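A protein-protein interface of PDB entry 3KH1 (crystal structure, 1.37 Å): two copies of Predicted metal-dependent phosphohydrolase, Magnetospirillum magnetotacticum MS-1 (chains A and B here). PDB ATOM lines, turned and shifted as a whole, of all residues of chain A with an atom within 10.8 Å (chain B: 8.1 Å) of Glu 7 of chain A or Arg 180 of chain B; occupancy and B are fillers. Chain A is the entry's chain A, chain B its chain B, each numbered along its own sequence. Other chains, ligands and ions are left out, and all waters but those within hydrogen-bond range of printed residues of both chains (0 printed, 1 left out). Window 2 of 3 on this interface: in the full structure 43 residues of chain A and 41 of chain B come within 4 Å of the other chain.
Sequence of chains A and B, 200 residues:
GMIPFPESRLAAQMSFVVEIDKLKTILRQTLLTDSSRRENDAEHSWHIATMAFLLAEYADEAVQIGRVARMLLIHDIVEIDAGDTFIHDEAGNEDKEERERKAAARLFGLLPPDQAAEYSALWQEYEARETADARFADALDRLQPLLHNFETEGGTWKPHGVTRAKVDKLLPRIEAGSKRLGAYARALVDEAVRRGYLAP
The side-chain hydroxyl (OH) of Tyr 58 of chain B sits at hydrogen-bond distance from the side-chain amide oxygen (OE1) of Gln 13 of chain A, at 2.6 Å.
OE1 of Glu 7 of chain A lies within salt-bridge range of NH2 of Arg 180 of chain B (2.9 Å).
The guanidinium group (NE) of Arg 9 of chain A is in salt-bridge range of the side-chain carboxylate (OE2) of Glu 57 of chain B, at 2.9 Å.
The side-chain amide nitrogen of Gln 13 of chain A lies within hydrogen-bond range of the side-chain carboxylate of Glu 57 of chain B (2.9 Å).
OG of Ser 178 of chain B is in hydrogen-bond range of N of Leu 181 of chain B (3.1 Å).
The side-chain hydroxyl of Ser 178 of chain B lies close to the backbone NH of Arg 180 of chain B (3.3 Å).
O of Tyr 58 of chain B is in hydrogen-bond range of OG of Ser 178 of chain B.
Tyr 58 of chain B touches Leu 10 of chain A (CE2 to CD1, 3.7 Å).
NH2 of Arg 180 of chain B touches CD2 of Leu 10 of chain A (3.6 Å).
Leu 10 of chain A touches Tyr 184 of chain B.
Met 14 of chain A touches Leu 143 of chain B (CE to CD2, 3.7 Å).
CD2 of Leu 181 of chain B touches CE of Met 14 of chain A, at 3.8 Å.
Met 14 of chain A touches Tyr 184 of chain B.
Ile 3 of chain A touches none of the printed residues of chain B.
Glu 7 of chain A touches just one residue of chain B: Arg 180.
Of the printed residues of chain B, Arg 9 of chain A touches Glu 57.
Of the printed residues of chain B, Leu 10 of chain A touches Tyr 58, Arg 180 and Tyr 184.
Of the printed residues of chain A, Tyr 58 of chain B touches Leu 10 (3.7 Å) and Gln 13 (2.6 Å).
No residue of chain A comes within 4 Å of Ser 178 of chain B.
Of the printed residues of chain A, Arg 180 of chain B touches Glu 7 (2.9 Å) and Leu 10 (3.6 Å).
Leu 181 of chain B touches one residue of chain A.
The nearest residue of chain B that does not touch Glu 7 of chain A is Tyr 184 of chain B (4.8 Å).
The nearest residue of chain A that does not touch Arg 180 of chain B is Pro 6 of chain A (4.3 Å).
The nearest printed residue of chain A that does not touch Glu 57 of chain B is Pro 112 of chain A (6.3 Å).
Of the 17 printed residues of chain A, 5 touch a printed residue of chain B.
Printed residues of chain A that touch a printed residue of chain B: Glu 7, Arg 9, Leu 10, Gln 13 and Met 14.
No position is printed for both chains.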
ATOM      1  N   MET A   2     -33.333  -2.365  -5.177  1.00  0.00           N
ATOM      2  CA  MET A   2     -32.132  -2.060  -4.330  1.00  0.00           C
ATOM      3  C   MET A   2     -31.039  -3.148  -4.520  1.00  0.00           C
ATOM      4  O   MET A   2     -31.195  -4.306  -4.097  1.00  0.00           O
ATOM      5  CB  MET A   2     -32.526  -1.842  -2.844  1.00  0.00           C
ATOM      6  CG  MET A   2     -33.064  -0.401  -2.521  1.00  0.00           C
ATOM      7  SD  MET A   2     -34.002  -0.127  -0.777  1.00  0.00           S
ATOM      8  CE  MET A   2     -34.585  -1.983  -0.525  1.00  0.00           C
ATOM      9  N   ILE A   3     -29.950  -2.719  -5.178  1.00  0.00           N
ATOM     10  CA  ILE A   3     -28.816  -3.462  -5.554  1.00  0.00           C
ATOM     11  C   ILE A   3     -27.765  -3.117  -4.507  1.00  0.00           C
ATOM     12  O   ILE A   3     -27.307  -1.967  -4.440  1.00  0.00           O
ATOM     13  CB  ILE A   3     -28.374  -3.023  -6.976  1.00  0.00           C
ATOM     14  CG1 ILE A   3     -29.533  -3.192  -7.977  1.00  0.00           C
ATOM     15  CG2 ILE A   3     -27.144  -3.804  -7.449  1.00  0.00           C
ATOM     16  CD1 ILE A   3     -29.207  -2.724  -9.404  1.00  0.00           C
ATOM     17  N   PRO A   4     -27.409  -4.086  -3.663  1.00  0.00           N
ATOM     18  CA  PRO A   4     -26.410  -3.764  -2.659  1.00  0.00           C
ATOM     19  C   PRO A   4     -25.105  -3.342  -3.280  1.00  0.00           C
ATOM     20  O   PRO A   4     -24.816  -3.690  -4.458  1.00  0.00           O
ATOM     21  CB  PRO A   4     -26.242  -5.088  -1.880  1.00  0.00           C
ATOM     22  CG  PRO A   4     -27.531  -5.826  -2.159  1.00  0.00           C
ATOM     23  CD  PRO A   4     -27.888  -5.478  -3.534  1.00  0.00           C
ATOM     24  N   PHE A   5     -24.300  -2.618  -2.515  1.00  0.00           N
ATOM     25  CA  PHE A   5     -23.056  -2.116  -3.079  1.00  0.00           C
ATOM     26  C   PHE A   5     -22.158  -3.202  -3.695  1.00  0.00           C
ATOM     27  O   PHE A   5     -21.655  -2.982  -4.794  1.00  0.00           O
ATOM     28  CB  PHE A   5     -22.338  -1.268  -2.007  1.00  0.00           C
ATOM     29  CG  PHE A   5     -21.002  -0.764  -2.442  1.00  0.00           C
ATOM     30  CD1 PHE A   5     -20.875   0.069  -3.526  1.00  0.00           C
ATOM     31  CD2 PHE A   5     -19.864  -1.126  -1.762  1.00  0.00           C
ATOM     32  CE1 PHE A   5     -19.608   0.499  -3.952  1.00  0.00           C
ATOM     33  CE2 PHE A   5     -18.619  -0.664  -2.154  1.00  0.00           C
ATOM     34  CZ  PHE A   5     -18.498   0.149  -3.248  1.00  0.00           C
ATOM     35  N   PRO A   6     -22.000  -4.395  -3.059  1.00  0.00           N
ATOM     36  CA  PRO A   6     -21.154  -5.416  -3.677  1.00  0.00           C
ATOM     37  C   PRO A   6     -21.652  -5.985  -4.986  1.00  0.00           C
ATOM     38  O   PRO A   6     -20.887  -6.618  -5.693  1.00  0.00           O
ATOM     39  CB  PRO A   6     -21.148  -6.549  -2.638  1.00  0.00           C
ATOM     40  CG  PRO A   6     -21.437  -5.902  -1.387  1.00  0.00           C
ATOM     41  CD  PRO A   6     -22.438  -4.820  -1.712  1.00  0.00           C
ATOM     42  N   GLU A   7     -22.930  -5.778  -5.310  1.00  0.00           N
ATOM     43  CA  GLU A   7     -23.505  -6.257  -6.546  1.00  0.00           C
ATOM     44  C   GLU A   7     -23.381  -5.252  -7.700  1.00  0.00           C
ATOM     45  O   GLU A   7     -23.920  -5.489  -8.784  1.00  0.00           O
ATOM     46  CB  GLU A   7     -24.957  -6.599  -6.291  1.00  0.00           C
ATOM     47  CG  GLU A   7     -25.176  -7.805  -5.419  1.00  0.00           C
ATOM     48  CD  GLU A   7     -24.876  -9.120  -6.099  1.00  0.00           C
ATOM     49  OE1 GLU A   7     -24.992  -9.229  -7.357  1.00  0.00           O
ATOM     50  OE2 GLU A   7     -24.519 -10.042  -5.323  1.00  0.00           O
ATOM     51  N   SER A   8     -22.687  -4.131  -7.461  1.00  0.00           N
ATOM     52  CA  SER A   8     -22.640  -3.023  -8.418  1.00  0.00           C
ATOM     53  C   SER A   8     -21.988  -3.419  -9.731  1.00  0.00           C
ATOM     54  O   SER A   8     -22.479  -3.062 -10.789  1.00  0.00           O
ATOM     55  CB  SER A   8     -21.864  -1.841  -7.834  1.00  0.00           C
ATOM     56  OG  SER A   8     -22.542  -1.300  -6.720  1.00  0.00           O
ATOM     57  N   ARG A   9     -20.888  -4.145  -9.646  1.00  0.00           N
ATOM     58  CA  ARG A   9     -20.155  -4.468 -10.871  1.00  0.00           C
ATOM     59  C   ARG A   9     -21.008  -5.332 -11.797  1.00  0.00           C
ATOM     60  O   ARG A   9     -21.127  -5.045 -12.988  1.00  0.00           O
ATOM     61  CB  ARG A   9     -18.837  -5.167 -10.501  1.00  0.00           C
ATOM     62  CG  ARG A   9     -18.069  -5.701 -11.716  1.00  0.00           C
ATOM     63  CD  ARG A   9     -16.728  -6.271 -11.279  1.00  0.00           C
ATOM     64  NE  ARG A   9     -16.002  -6.781 -12.430  1.00  0.00           N
ATOM     65  CZ  ARG A   9     -15.284  -6.026 -13.265  1.00  0.00           C
ATOM     66  NH1 ARG A   9     -15.113  -4.735 -13.059  1.00  0.00           N
ATOM     67  NH2 ARG A   9     -14.701  -6.569 -14.321  1.00  0.00           N
ATOM     68  N   LEU A  10     -21.594  -6.397 -11.258  1.00  0.00           N
ATOM     69  CA  LEU A  10     -22.397  -7.322 -12.063  1.00  0.00           C
ATOM     70  C   LEU A  10     -23.632  -6.544 -12.571  1.00  0.00           C
ATOM     71  O   LEU A  10     -24.047  -6.754 -13.701  1.00  0.00           O
ATOM     72  CB  LEU A  10     -22.754  -8.566 -11.252  1.00  0.00           C
ATOM     73  CG  LEU A  10     -23.541  -9.621 -12.033  1.00  0.00           C
ATOM     74  CD1 LEU A  10     -22.857 -10.073 -13.340  1.00  0.00           C
ATOM     75  CD2 LEU A  10     -23.827 -10.799 -11.094  1.00  0.00           C
ATOM     76  N   ALA A  11     -24.252  -5.691 -11.749  1.00  0.00           N
ATOM     77  CA  ALA A  11     -25.410  -4.956 -12.239  1.00  0.00           C
ATOM     78  C   ALA A  11     -25.046  -4.049 -13.418  1.00  0.00           C
ATOM     79  O   ALA A  11     -25.838  -3.933 -14.359  1.00  0.00           O
ATOM     80  CB  ALA A  11     -26.019  -4.138 -11.120  1.00  0.00           C
ATOM     81  N   ALA A  12     -23.874  -3.432 -13.378  1.00  0.00           N
ATOM     82  CA  ALA A  12     -23.426  -2.567 -14.462  1.00  0.00           C
ATOM     83  C   ALA A  12     -23.217  -3.405 -15.716  1.00  0.00           C
ATOM     84  O   ALA A  12     -23.693  -3.062 -16.816  1.00  0.00           O
ATOM     85  CB  ALA A  12     -22.138  -1.807 -14.077  1.00  0.00           C
ATOM     86  N   GLN A  13     -22.561  -4.561 -15.566  1.00  0.00           N
ATOM     87  CA  GLN A  13     -22.380  -5.478 -16.698  1.00  0.00           C
ATOM     88  C   GLN A  13     -23.708  -5.916 -17.314  1.00  0.00           C
ATOM     89  O   GLN A  13     -23.878  -5.891 -18.534  1.00  0.00           O
ATOM     90  CB  GLN A  13     -21.541  -6.689 -16.269  1.00  0.00           C
ATOM     91  CG  GLN A  13     -20.132  -6.278 -15.918  1.00  0.00           C
ATOM     92  CD  GLN A  13     -19.367  -7.345 -15.141  1.00  0.00           C
ATOM     93  OE1 GLN A  13     -19.956  -8.076 -14.332  1.00  0.00           O
ATOM     94  NE2 GLN A  13     -18.039  -7.474 -15.425  1.00  0.00           N
ATOM     95  N   MET A  14     -24.687  -6.253 -16.477  1.00  0.00           N
ATOM     96  CA  MET A  14     -25.986  -6.682 -16.998  1.00  0.00           C
ATOM     97  C   MET A  14     -26.719  -5.538 -17.671  1.00  0.00           C
ATOM     98  O   MET A  14     -27.386  -5.757 -18.689  1.00  0.00           O
ATOM     99  CB  MET A  14     -26.876  -7.266 -15.897  1.00  0.00           C
ATOM    100  CG  MET A  14     -26.331  -8.519 -15.288  1.00  0.00           C
ATOM    101  SD  MET A  14     -25.906  -9.913 -16.589  1.00  0.00           S
ATOM    102  CE  MET A  14     -25.636 -11.304 -15.336  1.00  0.00           C
ATOM    103  N   SER A  15     -26.557  -4.305 -17.159  1.00  0.00           N
ATOM    104  CA  SER A  15     -27.200  -3.155 -17.780  1.00  0.00           C
ATOM    105  C   SER A  15     -26.699  -2.952 -19.230  1.00  0.00           C
ATOM    106  O   SER A  15     -27.492  -2.655 -20.129  1.00  0.00           O
ATOM    107  CB  SER A  15     -27.009  -1.913 -16.941  1.00  0.00           C
ATOM    108  OG  SER A  15     -25.740  -1.283 -17.112  1.00  0.00           O
ATOM    109  N   LEU A 110     -21.780   2.433 -19.532  1.00  0.00           N
ATOM    110  CA  LEU A 110     -22.625   1.560 -18.705  1.00  0.00           C
ATOM    111  C   LEU A 110     -21.804   0.479 -17.970  1.00  0.00           C
ATOM    112  O   LEU A 110     -22.199  -0.015 -16.924  1.00  0.00           O
ATOM    113  CB  LEU A 110     -23.710   0.897 -19.551  1.00  0.00           C
ATOM    114  CG  LEU A 110     -24.788   1.829 -20.144  1.00  0.00           C
ATOM    115  CD1 LEU A 110     -25.688   1.044 -21.110  1.00  0.00           C
ATOM    116  CD2 LEU A 110     -25.612   2.533 -19.038  1.00  0.00           C
ATOM    117  N   LEU A 111     -20.694   0.070 -18.564  1.00  0.00           N
ATOM    118  CA  LEU A 111     -19.871  -0.992 -17.990  1.00  0.00           C
ATOM    119  C   LEU A 111     -19.134  -0.494 -16.749  1.00  0.00           C
ATOM    120  O   LEU A 111     -18.971   0.716 -16.564  1.00  0.00           O
ATOM    121  CB  LEU A 111     -18.858  -1.491 -19.028  1.00  0.00           C
ATOM    122  CG  LEU A 111     -19.464  -2.282 -20.189  1.00  0.00           C
ATOM    123  CD1 LEU A 111     -18.470  -2.313 -21.359  1.00  0.00           C
ATOM    124  CD2 LEU A 111     -19.895  -3.673 -19.704  1.00  0.00           C
ATOM    125  N   PRO A 112     -18.659  -1.433 -15.913  1.00  0.00           N
ATOM    126  CA  PRO A 112     -17.732  -1.009 -14.877  1.00  0.00           C
ATOM    127  C   PRO A 112     -16.528  -0.273 -15.493  1.00  0.00           C
ATOM    128  O   PRO A 112     -16.185  -0.539 -16.641  1.00  0.00           O
ATOM    129  CB  PRO A 112     -17.272  -2.307 -14.219  1.00  0.00           C
ATOM    130  CG  PRO A 112     -18.075  -3.362 -14.780  1.00  0.00           C
ATOM    131  CD  PRO A 112     -18.833  -2.890 -15.958  1.00  0.00           C
ATOM    132  N   GLU B  57     -15.192 -13.305 -16.426  1.00  0.00           N
ATOM    133  CA  GLU B  57     -14.656 -13.424 -15.084  1.00  0.00           C
ATOM    134  C   GLU B  57     -15.435 -14.412 -14.202  1.00  0.00           C
ATOM    135  O   GLU B  57     -14.950 -14.846 -13.170  1.00  0.00           O
ATOM    136  CB  GLU B  57     -14.582 -12.048 -14.393  1.00  0.00           C
ATOM    137  CG  GLU B  57     -15.918 -11.491 -13.940  1.00  0.00           C
ATOM    138  CD  GLU B  57     -15.792 -10.017 -13.641  1.00  0.00           C
ATOM    139  OE1 GLU B  57     -15.865  -9.226 -14.589  1.00  0.00           O
ATOM    140  OE2 GLU B  57     -15.598  -9.641 -12.459  1.00  0.00           O
ATOM    141  N   TYR B  58     -16.665 -14.686 -14.588  1.00  0.00           N
ATOM    142  CA  TYR B  58     -17.558 -15.583 -13.861  1.00  0.00           C
ATOM    143  C   TYR B  58     -17.452 -17.059 -14.264  1.00  0.00           C
ATOM    144  O   TYR B  58     -18.056 -17.917 -13.610  1.00  0.00           O
ATOM    145  CB  TYR B  58     -19.039 -15.091 -13.947  1.00  0.00           C
ATOM    146  CG  TYR B  58     -19.132 -13.639 -13.497  1.00  0.00           C
ATOM    147  CD1 TYR B  58     -18.921 -13.253 -12.191  1.00  0.00           C
ATOM    148  CD2 TYR B  58     -19.404 -12.640 -14.407  1.00  0.00           C
ATOM    149  CE1 TYR B  58     -18.936 -11.906 -11.812  1.00  0.00           C
ATOM    150  CE2 TYR B  58     -19.433 -11.320 -14.040  1.00  0.00           C
ATOM    151  CZ  TYR B  58     -19.214 -10.938 -12.728  1.00  0.00           C
ATOM    152  OH  TYR B  58     -19.239  -9.599 -12.344  1.00  0.00           O
ATOM    153  N   ALA B  59     -16.648 -17.338 -15.278  1.00  0.00           N
ATOM    154  CA  ALA B  59     -16.406 -18.706 -15.703  1.00  0.00           C
ATOM    155  C   ALA B  59     -15.377 -19.403 -14.814  1.00  0.00           C
ATOM    156  O   ALA B  59     -14.449 -18.792 -14.262  1.00  0.00           O
ATOM    157  CB  ALA B  59     -15.884 -18.749 -17.172  1.00  0.00           C
ATOM    158  N   LEU B 143     -29.240 -17.817 -19.503  1.00  0.00           N
ATOM    159  CA  LEU B 143     -29.358 -16.579 -18.768  1.00  0.00           C
ATOM    160  C   LEU B 143     -30.011 -15.464 -19.557  1.00  0.00           C
ATOM    161  O   LEU B 143     -30.812 -14.688 -19.014  1.00  0.00           O
ATOM    162  CB  LEU B 143     -27.980 -16.174 -18.228  1.00  0.00           C
ATOM    163  CG  LEU B 143     -27.928 -14.817 -17.487  1.00  0.00           C
ATOM    164  CD1 LEU B 143     -28.682 -14.805 -16.165  1.00  0.00           C
ATOM    165  CD2 LEU B 143     -26.441 -14.416 -17.196  1.00  0.00           C
ATOM    166  N   ILE B 174     -27.744 -22.788 -15.533  1.00  0.00           N
ATOM    167  CA  ILE B 174     -26.984 -21.566 -15.332  1.00  0.00           C
ATOM    168  C   ILE B 174     -25.991 -21.771 -14.194  1.00  0.00           C
ATOM    169  O   ILE B 174     -24.830 -21.441 -14.320  1.00  0.00           O
ATOM    170  CB  ILE B 174     -27.891 -20.340 -15.059  1.00  0.00           C
ATOM    171  CG1 ILE B 174     -28.879 -20.140 -16.218  1.00  0.00           C
ATOM    172  CG2 ILE B 174     -27.036 -19.057 -14.851  1.00  0.00           C
ATOM    173  CD1 ILE B 174     -29.918 -19.062 -16.018  1.00  0.00           C
ATOM    174  N   GLU B 175     -26.463 -22.379 -13.108  1.00  0.00           N
ATOM    175  CA  GLU B 175     -25.615 -22.666 -11.967  1.00  0.00           C
ATOM    176  C   GLU B 175     -24.413 -23.532 -12.393  1.00  0.00           C
ATOM    177  O   GLU B 175     -23.285 -23.334 -11.869  1.00  0.00           O
ATOM    178  CB  GLU B 175     -26.432 -23.335 -10.842  1.00  0.00           C
ATOM    179  CG  GLU B 175     -27.478 -22.406 -10.195  1.00  0.00           C
ATOM    180  CD  GLU B 175     -28.537 -23.133  -9.382  1.00  0.00           C
ATOM    181  OE1 GLU B 175     -28.699 -24.366  -9.498  1.00  0.00           O
ATOM    182  OE2 GLU B 175     -29.236 -22.442  -8.629  1.00  0.00           O
ATOM    183  N   GLY B 177     -22.751 -23.483 -15.069  1.00  0.00           N
ATOM    184  CA  GLY B 177     -21.764 -22.638 -15.714  1.00  0.00           C
ATOM    185  C   GLY B 177     -21.131 -21.598 -14.795  1.00  0.00           C
ATOM    186  O   GLY B 177     -19.993 -21.164 -15.008  1.00  0.00           O
ATOM    187  N   SER B 178     -21.859 -21.141 -13.779  1.00  0.00           N
ATOM    188  CA  SER B 178     -21.340 -20.141 -12.864  1.00  0.00           C
ATOM    189  C   SER B 178     -22.230 -20.029 -11.659  1.00  0.00           C
ATOM    190  O   SER B 178     -23.413 -19.742 -11.801  1.00  0.00           O
ATOM    191  CB  SER B 178     -21.298 -18.782 -13.544  1.00  0.00           C
ATOM    192  OG  SER B 178     -21.021 -17.762 -12.612  1.00  0.00           O
ATOM    193  N   LYS B 179     -21.660 -20.234 -10.472  1.00  0.00           N
ATOM    194  CA  LYS B 179     -22.428 -20.098  -9.234  1.00  0.00           C
ATOM    195  C   LYS B 179     -22.957 -18.680  -9.061  1.00  0.00           C
ATOM    196  O   LYS B 179     -24.087 -18.481  -8.646  1.00  0.00           O
ATOM    197  CB  LYS B 179     -21.598 -20.569  -8.057  1.00  0.00           C
ATOM    198  CG  LYS B 179     -21.461 -22.080  -8.064  1.00  0.00           C
ATOM    199  N   ARG B 180     -22.147 -17.701  -9.462  1.00  0.00           N
ATOM    200  CA  ARG B 180     -22.524 -16.318  -9.315  1.00  0.00           C
ATOM    201  C   ARG B 180     -23.672 -15.976 -10.259  1.00  0.00           C
ATOM    202  O   ARG B 180     -24.636 -15.344  -9.851  1.00  0.00           O
ATOM    203  CB  ARG B 180     -21.328 -15.426  -9.593  1.00  0.00           C
ATOM    204  CG  ARG B 180     -21.619 -13.966  -9.446  1.00  0.00           C
ATOM    205  CD  ARG B 180     -21.840 -13.605  -7.978  1.00  0.00           C
ATOM    206  NE  ARG B 180     -22.385 -12.260  -7.874  1.00  0.00           N
ATOM    207  CZ  ARG B 180     -21.664 -11.154  -7.991  1.00  0.00           C
ATOM    208  NH1 ARG B 180     -20.359 -11.226  -8.209  1.00  0.00           N
ATOM    209  NH2 ARG B 180     -22.266  -9.974  -7.920  1.00  0.00           N
ATOM    210  N   LEU B 181     -23.576 -16.380 -11.532  1.00  0.00           N
ATOM    211  CA  LEU B 181     -24.650 -16.105 -12.468  1.00  0.00           C
ATOM    212  C   LEU B 181     -25.920 -16.884 -12.085  1.00  0.00           C
ATOM    213  O   LEU B 181     -27.015 -16.414 -12.293  1.00  0.00           O
ATOM    214  CB  LEU B 181     -24.188 -16.435 -13.897  1.00  0.00           C
ATOM    215  CG  LEU B 181     -23.003 -15.590 -14.446  1.00  0.00           C
ATOM    216  CD1 LEU B 181     -22.796 -15.922 -15.881  1.00  0.00           C
ATOM    217  CD2 LEU B 181     -23.250 -14.062 -14.276  1.00  0.00           C
ATOM    218  N   GLY B 182     -25.766 -18.086 -11.547  1.00  0.00           N
ATOM    219  CA  GLY B 182     -26.874 -18.861 -11.033  1.00  0.00           C
ATOM    220  C   GLY B 182     -27.631 -18.153  -9.941  1.00  0.00           C
ATOM    221  O   GLY B 182     -28.872 -18.102  -9.931  1.00  0.00           O
ATOM    222  N   ALA B 183     -26.883 -17.579  -9.021  1.00  0.00           N
ATOM    223  CA  ALA B 183     -27.477 -16.817  -7.921  1.00  0.00           C
ATOM    224  C   ALA B 183     -28.204 -15.581  -8.438  1.00  0.00           C
ATOM    225  O   ALA B 183     -29.303 -15.255  -7.975  1.00  0.00           O
ATOM    226  CB  ALA B 183     -26.427 -16.426  -6.892  1.00  0.00           C
ATOM    227  N   TYR B 184     -27.596 -14.907  -9.414  1.00  0.00           N
ATOM    228  CA  TYR B 184     -28.247 -13.752 -10.021  1.00  0.00           C
ATOM    229  C   TYR B 184     -29.581 -14.203 -10.650  1.00  0.00           C
ATOM    230  O   TYR B 184     -30.619 -13.540 -10.492  1.00  0.00           O
ATOM    231  CB  TYR B 184     -27.313 -13.137 -11.059  1.00  0.00           C
ATOM    232  CG  TYR B 184     -27.855 -11.888 -11.710  1.00  0.00           C
ATOM    233  CD1 TYR B 184     -28.674 -11.974 -12.828  1.00  0.00           C
ATOM    234  CD2 TYR B 184     -27.557 -10.618 -11.209  1.00  0.00           C
ATOM    235  CE1 TYR B 184     -29.197 -10.868 -13.411  1.00  0.00           C
ATOM    236  CE2 TYR B 184     -28.096  -9.485 -11.808  1.00  0.00           C
ATOM    237  CZ  TYR B 184     -28.899  -9.616 -12.904  1.00  0.00           C
ATOM    238  OH  TYR B 184     -29.436  -8.515 -13.502  1.00  0.00           O
ATOM    239  N   ALA B 185     -29.530 -15.306 -11.402  1.00  0.00           N
ATOM    240  CA  ALA B 185     -30.700 -15.801 -12.097  1.00  0.00           C
ATOM    241  C   ALA B 185     -31.820 -16.169 -11.100  1.00  0.00           C
ATOM    242  O   ALA B 185     -33.001 -15.828 -11.329  1.00  0.00           O
ATOM    243  CB  ALA B 185     -30.322 -16.963 -12.955  1.00  0.00           C
ATOM    244  N   ARG B 186     -31.472 -16.846 -10.004  1.00  0.00           N
ATOM    245  CA  ARG B 186     -32.476 -17.217  -9.000  1.00  0.00           C
ATOM    246  C   ARG B 186     -33.165 -15.985  -8.428  1.00  0.00           C
ATOM    247  O   ARG B 186     -34.398 -15.958  -8.298  1.00  0.00           O
ATOM    248  CB  ARG B 186     -31.869 -18.057  -7.877  1.00  0.00           C
ATOM    249  CG  ARG B 186     -31.360 -19.401  -8.376  1.00  0.00           C
ATOM    250  CD  ARG B 186     -31.676 -20.520  -7.395  1.00  0.00           C
ATOM    251  NE  ARG B 186     -31.487 -21.824  -8.015  1.00  0.00           N
ATOM    252  CZ  ARG B 186     -32.459 -22.710  -8.168  1.00  0.00           C
ATOM    253  NH1 ARG B 186     -33.675 -22.416  -7.735  1.00  0.00           N
ATOM    254  NH2 ARG B 186     -32.210 -23.884  -8.733  1.00  0.00           N
ATOM    255  N   ALA B 187     -32.386 -14.955  -8.081  1.00  0.00           N
ATOM    256  CA  ALA B 187     -32.953 -13.731  -7.522  1.00  0.00           C
ATOM    257  C   ALA B 187     -33.837 -13.039  -8.549  1.00  0.00           C
ATOM    258  O   ALA B 187     -34.886 -12.504  -8.215  1.00  0.00           O
ATOM    259  CB  ALA B 187     -31.825 -12.775  -7.046  1.00  0.00           C
